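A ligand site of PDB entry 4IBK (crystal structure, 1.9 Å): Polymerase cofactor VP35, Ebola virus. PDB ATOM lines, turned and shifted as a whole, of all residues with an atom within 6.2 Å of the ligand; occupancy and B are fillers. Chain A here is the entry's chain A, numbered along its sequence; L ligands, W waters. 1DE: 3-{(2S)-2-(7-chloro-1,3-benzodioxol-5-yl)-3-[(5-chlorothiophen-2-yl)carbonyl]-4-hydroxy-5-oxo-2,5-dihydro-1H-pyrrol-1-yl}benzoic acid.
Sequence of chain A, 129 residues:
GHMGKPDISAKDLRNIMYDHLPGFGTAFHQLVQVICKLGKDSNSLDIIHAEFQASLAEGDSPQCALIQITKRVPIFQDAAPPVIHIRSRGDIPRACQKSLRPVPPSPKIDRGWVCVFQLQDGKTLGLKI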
ATOM      1  N   ALA A  10     -23.798  -6.106 -27.756  1.00  0.00           N
ATOM      2  CA  ALA A  10     -23.906  -5.007 -26.803  1.00  0.00           C
ATOM      3  C   ALA A  10     -22.523  -4.459 -26.448  1.00  0.00           C
ATOM      4  O   ALA A  10     -22.335  -3.249 -26.370  1.00  0.00           O
ATOM      5  CB  ALA A  10     -24.627  -5.469 -25.548  1.00  0.00           C
ATOM      6  N   LYS A  11     -21.567  -5.344 -26.223  1.00  0.00           N
ATOM      7  CA  LYS A  11     -20.197  -4.928 -25.915  1.00  0.00           C
ATOM      8  C   LYS A  11     -19.561  -4.153 -27.070  1.00  0.00           C
ATOM      9  O   LYS A  11     -18.945  -3.108 -26.859  1.00  0.00           O
ATOM     10  CB  LYS A  11     -19.357  -6.139 -25.523  1.00  0.00           C
ATOM     11  CG  LYS A  11     -17.901  -5.820 -25.217  1.00  0.00           C
ATOM     12  CD  LYS A  11     -17.117  -7.110 -25.023  1.00  0.00           C
ATOM     13  CE  LYS A  11     -15.637  -6.835 -24.847  1.00  0.00           C
ATOM     14  NZ  LYS A  11     -15.400  -5.904 -23.700  1.00  0.00           N
ATOM     15  N   ARG A  14     -21.241  -0.676 -27.227  1.00  0.00           N
ATOM     16  CA  ARG A  14     -20.748   0.107 -26.103  1.00  0.00           C
ATOM     17  C   ARG A  14     -19.381   0.724 -26.429  1.00  0.00           C
ATOM     18  O   ARG A  14     -19.146   1.927 -26.225  1.00  0.00           O
ATOM     19  CB  ARG A  14     -20.635  -0.778 -24.854  1.00  0.00           C
ATOM     20  CG  ARG A  14     -20.337  -0.018 -23.561  1.00  0.00           C
ATOM     21  CD  ARG A  14     -19.899  -0.989 -22.483  1.00  0.00           C
ATOM     22  NE  ARG A  14     -18.539  -1.453 -22.742  1.00  0.00           N
ATOM     23  CZ  ARG A  14     -17.986  -2.518 -22.195  1.00  0.00           C
ATOM     24  NH1 ARG A  14     -18.681  -3.277 -21.342  1.00  0.00           N
ATOM     25  NH2 ARG A  14     -16.740  -2.846 -22.507  1.00  0.00           N
ATOM     26  N   GLN A  30     -22.857   6.114 -18.882  1.00  0.00           N
ATOM     27  CA  GLN A  30     -23.925   5.295 -18.312  1.00  0.00           C
ATOM     28  C   GLN A  30     -25.121   5.219 -19.268  1.00  0.00           C
ATOM     29  O   GLN A  30     -25.770   4.179 -19.360  1.00  0.00           O
ATOM     30  CB  GLN A  30     -24.351   5.819 -16.942  1.00  0.00           C
ATOM     31  CG  GLN A  30     -25.306   4.920 -16.221  1.00  0.00           C
ATOM     32  CD  GLN A  30     -24.810   3.489 -16.060  1.00  0.00           C
ATOM     33  OE1 GLN A  30     -23.604   3.232 -15.997  1.00  0.00           O
ATOM     34  NE2 GLN A  30     -25.746   2.550 -15.983  1.00  0.00           N
ATOM     35  N   GLN A  33     -24.429   2.516 -21.572  1.00  0.00           N
ATOM     36  CA  GLN A  33     -24.678   1.234 -20.919  1.00  0.00           C
ATOM     37  C   GLN A  33     -26.155   0.862 -20.958  1.00  0.00           C
ATOM     38  O   GLN A  33     -26.518  -0.287 -21.234  1.00  0.00           O
ATOM     39  CB  GLN A  33     -24.252   1.308 -19.458  1.00  0.00           C
ATOM     40  CG  GLN A  33     -22.758   1.341 -19.250  1.00  0.00           C
ATOM     41  CD  GLN A  33     -22.175  -0.063 -19.154  1.00  0.00           C
ATOM     42  OE1 GLN A  33     -22.565  -0.962 -19.887  1.00  0.00           O
ATOM     43  NE2 GLN A  33     -21.240  -0.237 -18.243  1.00  0.00           N
ATOM     44  N   VAL A  34     -27.009   1.838 -20.674  1.00  0.00           N
ATOM     45  CA  VAL A  34     -28.446   1.617 -20.604  1.00  0.00           C
ATOM     46  C   VAL A  34     -29.020   1.335 -21.989  1.00  0.00           C
ATOM     47  O   VAL A  34     -29.862   0.444 -22.173  1.00  0.00           O
ATOM     48  CB  VAL A  34     -29.156   2.840 -19.972  1.00  0.00           C
ATOM     49  CG1 VAL A  34     -30.669   2.775 -20.194  1.00  0.00           C
ATOM     50  CG2 VAL A  34     -28.825   2.923 -18.491  1.00  0.00           C
ATOM     51  N   ILE A  35     -28.584   2.122 -22.963  1.00  0.00           N
ATOM     52  CA  ILE A  35     -29.014   1.951 -24.337  1.00  0.00           C
ATOM     53  C   ILE A  35     -28.617   0.579 -24.868  1.00  0.00           C
ATOM     54  O   ILE A  35     -29.400  -0.088 -25.538  1.00  0.00           O
ATOM     55  CB  ILE A  35     -28.431   3.063 -25.236  1.00  0.00           C
ATOM     56  CG1 ILE A  35     -29.177   4.367 -24.999  1.00  0.00           C
ATOM     57  CG2 ILE A  35     -28.502   2.667 -26.702  1.00  0.00           C
ATOM     58  CD1 ILE A  35     -28.471   5.601 -25.601  1.00  0.00           C
ATOM     59  N   CYS A  36     -27.412   0.127 -24.524  1.00  0.00           N
ATOM     60  CA  CYS A  36     -26.953  -1.168 -25.001  1.00  0.00           C
ATOM     61  C   CYS A  36     -27.665  -2.325 -24.312  1.00  0.00           C
ATOM     62  O   CYS A  36     -27.983  -3.334 -24.943  1.00  0.00           O
ATOM     63  CB  CYS A  36     -25.429  -1.309 -24.858  1.00  0.00           C
ATOM     64  SG  CYS A  36     -24.496  -0.204 -25.972  1.00  0.00           S
ATOM     65  N   LYS A  37     -27.932  -2.193 -23.013  1.00  0.00           N
ATOM     66  CA  LYS A  37     -28.581  -3.251 -22.267  1.00  0.00           C
ATOM     67  C   LYS A  37     -30.045  -3.395 -22.712  1.00  0.00           C
ATOM     68  O   LYS A  37     -30.521  -4.496 -23.007  1.00  0.00           O
ATOM     69  CB  LYS A  37     -28.470  -2.985 -20.752  1.00  0.00           C
ATOM     70  CG  LYS A  37     -29.330  -3.889 -19.856  1.00  0.00           C
ATOM     71  CD  LYS A  37     -28.910  -5.345 -19.967  1.00  0.00           C
ATOM     72  CE  LYS A  37     -29.478  -6.185 -18.807  1.00  0.00           C
ATOM     73  NZ  LYS A  37     -30.957  -6.077 -18.648  1.00  0.00           N
ATOM     74  N   LEU A  38     -30.741  -2.262 -22.801  1.00  0.00           N
ATOM     75  CA  LEU A  38     -32.150  -2.279 -23.213  1.00  0.00           C
ATOM     76  C   LEU A  38     -32.264  -2.648 -24.686  1.00  0.00           C
ATOM     77  O   LEU A  38     -33.212  -3.319 -25.102  1.00  0.00           O
ATOM     78  CB  LEU A  38     -32.834  -0.941 -22.939  1.00  0.00           C
ATOM     79  CG  LEU A  38     -33.008  -0.488 -21.480  1.00  0.00           C
ATOM     80  CD1 LEU A  38     -34.118   0.553 -21.378  1.00  0.00           C
ATOM     81  CD2 LEU A  38     -33.277  -1.664 -20.561  1.00  0.00           C
ATOM     82  N   LYS A  40     -30.106  -4.635 -26.252  1.00  0.00           N
ATOM     83  CA  LYS A  40     -29.846  -6.068 -26.318  1.00  0.00           C
ATOM     84  C   LYS A  40     -31.123  -6.852 -26.035  1.00  0.00           C
ATOM     85  O   LYS A  40     -31.501  -7.756 -26.774  1.00  0.00           O
ATOM     86  CB  LYS A  40     -28.758  -6.464 -25.322  1.00  0.00           C
ATOM     87  CG  LYS A  40     -28.450  -7.947 -25.279  1.00  0.00           C
ATOM     88  CD  LYS A  40     -27.334  -8.222 -24.287  1.00  0.00           C
ATOM     89  CE  LYS A  40     -26.936  -9.691 -24.308  1.00  0.00           C
ATOM     90  NZ  LYS A  40     -25.705  -9.922 -23.511  1.00  0.00           N
ATOM     91  N   ASP A  41     -31.815  -6.430 -24.965  1.00  0.00           N
ATOM     92  CA  ASP A  41     -32.978  -7.144 -24.454  1.00  0.00           C
ATOM     93  C   ASP A  41     -34.168  -7.046 -25.395  1.00  0.00           C
ATOM     94  O   ASP A  41     -35.116  -7.829 -25.291  1.00  0.00           O
ATOM     95  CB  ASP A  41     -33.365  -6.598 -23.072  1.00  0.00           C
ATOM     96  CG  ASP A  41     -32.370  -6.973 -21.975  1.00  0.00           C
ATOM     97  OD1 ASP A  41     -31.526  -7.881 -22.176  1.00  0.00           O
ATOM     98  OD2 ASP A  41     -32.447  -6.355 -20.887  1.00  0.00           O
ATOM     99  N   PRO A  82     -34.293   1.941 -16.305  1.00  0.00           N
ATOM    100  CA  PRO A  82     -34.091   0.647 -15.677  1.00  0.00           C
ATOM    101  C   PRO A  82     -33.581   0.856 -14.268  1.00  0.00           C
ATOM    102  O   PRO A  82     -32.956   1.873 -13.975  1.00  0.00           O
ATOM    103  CB  PRO A  82     -32.997   0.002 -16.532  1.00  0.00           C
ATOM    104  CG  PRO A  82     -32.262   1.177 -17.150  1.00  0.00           C
ATOM    105  CD  PRO A  82     -33.334   2.191 -17.406  1.00  0.00           C
ATOM    106  N   VAL A  83     -33.879  -0.101 -13.392  1.00  0.00           N
ATOM    107  CA  VAL A  83     -33.362  -0.070 -12.037  1.00  0.00           C
ATOM    108  C   VAL A  83     -32.079  -0.896 -12.008  1.00  0.00           C
ATOM    109  O   VAL A  83     -32.031  -2.018 -12.519  1.00  0.00           O
ATOM    110  CB  VAL A  83     -34.391  -0.629 -11.036  1.00  0.00           C
ATOM    111  CG1 VAL A  83     -33.782  -0.746  -9.629  1.00  0.00           C
ATOM    112  CG2 VAL A  83     -35.638   0.254 -11.016  1.00  0.00           C
ATOM    113  N   ILE A  84     -31.028  -0.315 -11.436  1.00  0.00           N
ATOM    114  CA  ILE A  84     -29.758  -1.001 -11.317  1.00  0.00           C
ATOM    115  C   ILE A  84     -29.389  -1.105  -9.852  1.00  0.00           C
ATOM    116  O   ILE A  84     -29.176  -0.105  -9.175  1.00  0.00           O
ATOM    117  CB  ILE A  84     -28.658  -0.258 -12.096  1.00  0.00           C
ATOM    118  CG1 ILE A  84     -29.028  -0.168 -13.586  1.00  0.00           C
ATOM    119  CG2 ILE A  84     -27.325  -0.939 -11.931  1.00  0.00           C
ATOM    120  CD1 ILE A  84     -28.036   0.633 -14.414  1.00  0.00           C
ATOM    121  N   HIS A  85     -29.315  -2.337  -9.341  1.00  0.00           N
ATOM    122  CA  HIS A  85     -29.004  -2.532  -7.930  1.00  0.00           C
ATOM    123  C   HIS A  85     -27.493  -2.417  -7.680  1.00  0.00           C
ATOM    124  O   HIS A  85     -26.701  -3.073  -8.341  1.00  0.00           O
ATOM    125  CB  HIS A  85     -29.526  -3.876  -7.428  1.00  0.00           C
ATOM    126  CG  HIS A  85     -29.508  -3.991  -5.933  1.00  0.00           C
ATOM    127  ND1 HIS A  85     -30.505  -3.461  -5.135  1.00  0.00           N
ATOM    128  CD2 HIS A  85     -28.595  -4.515  -5.092  1.00  0.00           C
ATOM    129  CE1 HIS A  85     -30.214  -3.679  -3.874  1.00  0.00           C
ATOM    130  NE2 HIS A  85     -29.056  -4.316  -3.806  1.00  0.00           N
ATOM    131  N   ILE A  86     -27.119  -1.584  -6.713  1.00  0.00           N
ATOM    132  CA  ILE A  86     -25.724  -1.403  -6.321  1.00  0.00           C
ATOM    133  C   ILE A  86     -25.604  -1.374  -4.810  1.00  0.00           C
ATOM    134  O   ILE A  86     -26.599  -1.211  -4.105  1.00  0.00           O
ATOM    135  CB  ILE A  86     -25.124  -0.092  -6.878  1.00  0.00           C
ATOM    136  CG1 ILE A  86     -25.878   1.109  -6.306  1.00  0.00           C
ATOM    137  CG2 ILE A  86     -25.174  -0.070  -8.402  1.00  0.00           C
ATOM    138  CD1 ILE A  86     -25.335   2.421  -6.790  1.00  0.00           C
ATOM    139  N   ASP A  91     -20.112   3.126  -5.561  1.00  0.00           N
ATOM    140  CA  ASP A  91     -19.976   2.247  -6.721  1.00  0.00           C
ATOM    141  C   ASP A  91     -20.247   2.976  -8.028  1.00  0.00           C
ATOM    142  O   ASP A  91     -19.922   2.483  -9.106  1.00  0.00           O
ATOM    143  CB  ASP A  91     -20.930   1.064  -6.594  1.00  0.00           C
ATOM    144  CG  ASP A  91     -20.646   0.253  -5.371  1.00  0.00           C
ATOM    145  OD1 ASP A  91     -19.459  -0.034  -5.128  1.00  0.00           O
ATOM    146  OD2 ASP A  91     -21.607  -0.090  -4.647  1.00  0.00           O
ATOM    147  N   ILE A  92     -20.875   4.149  -7.928  1.00  0.00           N
ATOM    148  CA  ILE A  92     -21.141   4.956  -9.108  1.00  0.00           C
ATOM    149  C   ILE A  92     -19.888   5.766  -9.447  1.00  0.00           C
ATOM    150  O   ILE A  92     -19.268   6.328  -8.546  1.00  0.00           O
ATOM    151  CB  ILE A  92     -22.343   5.887  -8.830  1.00  0.00           C
ATOM    152  CG1 ILE A  92     -23.544   5.051  -8.412  1.00  0.00           C
ATOM    153  CG2 ILE A  92     -22.685   6.744 -10.055  1.00  0.00           C
ATOM    154  CD1 ILE A  92     -24.787   5.861  -8.001  1.00  0.00           C
ATOM    155  N   PRO A  93     -19.508   5.809 -10.731  1.00  0.00           N
ATOM    156  CA  PRO A  93     -18.292   6.540 -11.122  1.00  0.00           C
ATOM    157  C   PRO A  93     -18.277   8.001 -10.658  1.00  0.00           C
ATOM    158  O   PRO A  93     -19.325   8.637 -10.611  1.00  0.00           O
ATOM    159  CB  PRO A  93     -18.326   6.457 -12.651  1.00  0.00           C
ATOM    160  CG  PRO A  93     -19.060   5.178 -12.934  1.00  0.00           C
ATOM    161  CD  PRO A  93     -20.145   5.155 -11.880  1.00  0.00           C
ATOM    162  N   CYS A 115     -31.045   6.140 -15.566  1.00  0.00           N
ATOM    163  CA  CYS A 115     -31.334   4.927 -14.822  1.00  0.00           C
ATOM    164  C   CYS A 115     -31.650   5.329 -13.399  1.00  0.00           C
ATOM    165  O   CYS A 115     -31.524   6.498 -13.029  1.00  0.00           O
ATOM    166  CB  CYS A 115     -30.151   3.951 -14.855  1.00  0.00           C
ATOM    167  SG  CYS A 115     -28.607   4.717 -14.307  1.00  0.00           S
ATOM    168  N   PHE A 117     -30.563   4.041  -9.590  1.00  0.00           N
ATOM    169  CA  PHE A 117     -29.739   3.179  -8.761  1.00  0.00           C
ATOM    170  C   PHE A 117     -30.516   2.849  -7.484  1.00  0.00           C
ATOM    171  O   PHE A 117     -30.998   3.744  -6.787  1.00  0.00           O
ATOM    172  CB  PHE A 117     -28.383   3.824  -8.452  1.00  0.00           C
ATOM    173  CG  PHE A 117     -27.513   3.977  -9.670  1.00  0.00           C
ATOM    174  CD1 PHE A 117     -27.283   5.232 -10.235  1.00  0.00           C
ATOM    175  CD2 PHE A 117     -26.947   2.860 -10.272  1.00  0.00           C
ATOM    176  CE1 PHE A 117     -26.473   5.363 -11.350  1.00  0.00           C
ATOM    177  CE2 PHE A 117     -26.138   2.984 -11.400  1.00  0.00           C
ATOM    178  CZ  PHE A 117     -25.909   4.230 -11.944  1.00  0.00           C
HETATM  179  CAO 1DE L   1     -26.650  -3.607 -16.060  1.00  0.00           C
HETATM  180  CBD 1DE L   1     -28.003  -3.694 -15.701  1.00  0.00           C
HETATM  181  OAQ 1DE L   1     -28.705  -4.527 -14.838  1.00  0.00           O
HETATM  182  CAP 1DE L   1     -30.042  -4.168 -14.878  1.00  0.00           C
HETATM  183  OAR 1DE L   1     -30.167  -3.063 -15.740  1.00  0.00           O
HETATM  184  CBF 1DE L   1     -28.897  -2.810 -16.234  1.00  0.00           C
HETATM  185  CAZ 1DE L   1     -28.461  -1.845 -17.139  1.00  0.00           C
HETATM  186 CL2  1DE L   1     -29.681  -0.790 -17.752  1.00  0.00          CL
HETATM  187  CAM 1DE L   1     -27.126  -1.740 -17.516  1.00  0.00           C
HETATM  188  CBB 1DE L   1     -26.220  -2.650 -16.969  1.00  0.00           C
HETATM  189  CBG 1DE L   1     -24.765  -2.644 -17.274  1.00  0.00           C
HETATM  190  CAX 1DE L   1     -23.978  -2.282 -16.187  1.00  0.00           C
HETATM  191  CAU 1DE L   1     -24.117  -0.974 -15.506  1.00  0.00           C
HETATM  192  OAB 1DE L   1     -24.599  -0.030 -16.122  1.00  0.00           O
HETATM  193  CBE 1DE L   1     -23.677  -0.729 -14.118  1.00  0.00           C
HETATM  194  CAL 1DE L   1     -23.355  -1.643 -13.104  1.00  0.00           C
HETATM  195  CAK 1DE L   1     -22.962  -1.022 -11.872  1.00  0.00           C
HETATM  196  CAY 1DE L   1     -22.993   0.376 -11.940  1.00  0.00           C
HETATM  197 CL1  1DE L   1     -22.616   1.508 -10.705  1.00  0.00          CL
HETATM  198  SAS 1DE L   1     -23.508   0.812 -13.471  1.00  0.00           S
HETATM  199  CAV 1DE L   1     -22.965  -3.247 -16.080  1.00  0.00           C
HETATM  200  OAE 1DE L   1     -21.977  -3.310 -15.127  1.00  0.00           O
HETATM  201  CAW 1DE L   1     -23.139  -4.137 -17.120  1.00  0.00           C
HETATM  202  OAC 1DE L   1     -22.377  -5.241 -17.413  1.00  0.00           O
HETATM  203  NBH 1DE L   1     -24.199  -3.734 -17.827  1.00  0.00           N
HETATM  204  CBC 1DE L   1     -24.596  -4.313 -19.067  1.00  0.00           C
HETATM  205  CAN 1DE L   1     -24.882  -5.668 -19.079  1.00  0.00           C
HETATM  206  CAJ 1DE L   1     -24.695  -3.550 -20.223  1.00  0.00           C
HETATM  207  CAH 1DE L   1     -25.082  -4.165 -21.394  1.00  0.00           C
HETATM  208  CAI 1DE L   1     -25.364  -5.534 -21.407  1.00  0.00           C
HETATM  209  CBA 1DE L   1     -25.261  -6.288 -20.248  1.00  0.00           C
HETATM  210  CAT 1DE L   1     -25.564  -7.749 -20.249  1.00  0.00           C
HETATM  211  OAD 1DE L   1     -25.916  -8.322 -21.305  1.00  0.00           O
HETATM  212  OAA 1DE L   1     -25.469  -8.409 -19.184  1.00  0.00           O
HETATM  213  O   HOH W   1     -28.997  -8.980 -20.621  1.00  0.00           O
HETATM  214  O   HOH W   2     -21.435   1.644 -16.139  1.00  0.00           O
HETATM  215  O   HOH W   3     -25.615  -7.427 -16.139  1.00  0.00           O
HETATM  216  O   HOH W   4     -32.565  -4.218 -17.140  1.00  0.00           O
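An oxygen (OAD) of the ligand is in salt-bridge range of the side-chain amino group of Lys 40, at 2.7 Å. The side-chain amide nitrogen (NE2) of Gln 30 lies within hydrogen-bond range of an oxygen (OAB) of the ligand (2.8 Å).
NZ of Lys 37 is in salt-bridge range of OD2 of Asp 41 (2.7 Å).
Gln 33 touches the ligand. CG2 of Val 34 touches CL2 of the ligand, 3.9 Å away. CG of Lys 37 touches CAZ of the ligand, 3.5 Å away. Pro 82 touches the ligand. Val 83 touches the ligand. Ile 84 touches the ligand (CD1 to CAZ, 3.7 Å). Ile 86 touches the ligand. O of Asp 91 touches CL1 of the ligand, at 3.3 Å. Phe 117 touches the ligand (CE2 to CL1, 3.9 Å). Hydrophobic or aromatic side chains within 4 Å of the ligand: Val 34, Pro 82, Ile 84, Ile 86 and Phe 117. 11 residues have an atom within 4 Å of the ligand: Gln 30, Gln 33, Val 34, Lys 37, Lys 40, Pro 82, Val 83, Ile 84, Ile 86, Asp 91 and Phe 117.
Water W4 lies within hydrogen-bond range of NZ of Lys 37 (2.9 Å) and OAR of the ligand (3.0 Å). Water W1 lies within hydrogen-bond range of the side-chain carboxylate of Asp 41 (3.2 Å) and an oxygen (OAD) of the ligand (3.2 Å). Water W2 lies within hydrogen-bond range of the side-chain amide oxygen of Gln 30, the side-chain amide nitrogen of Gln 33 and a sulfur (SAS) of the ligand.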
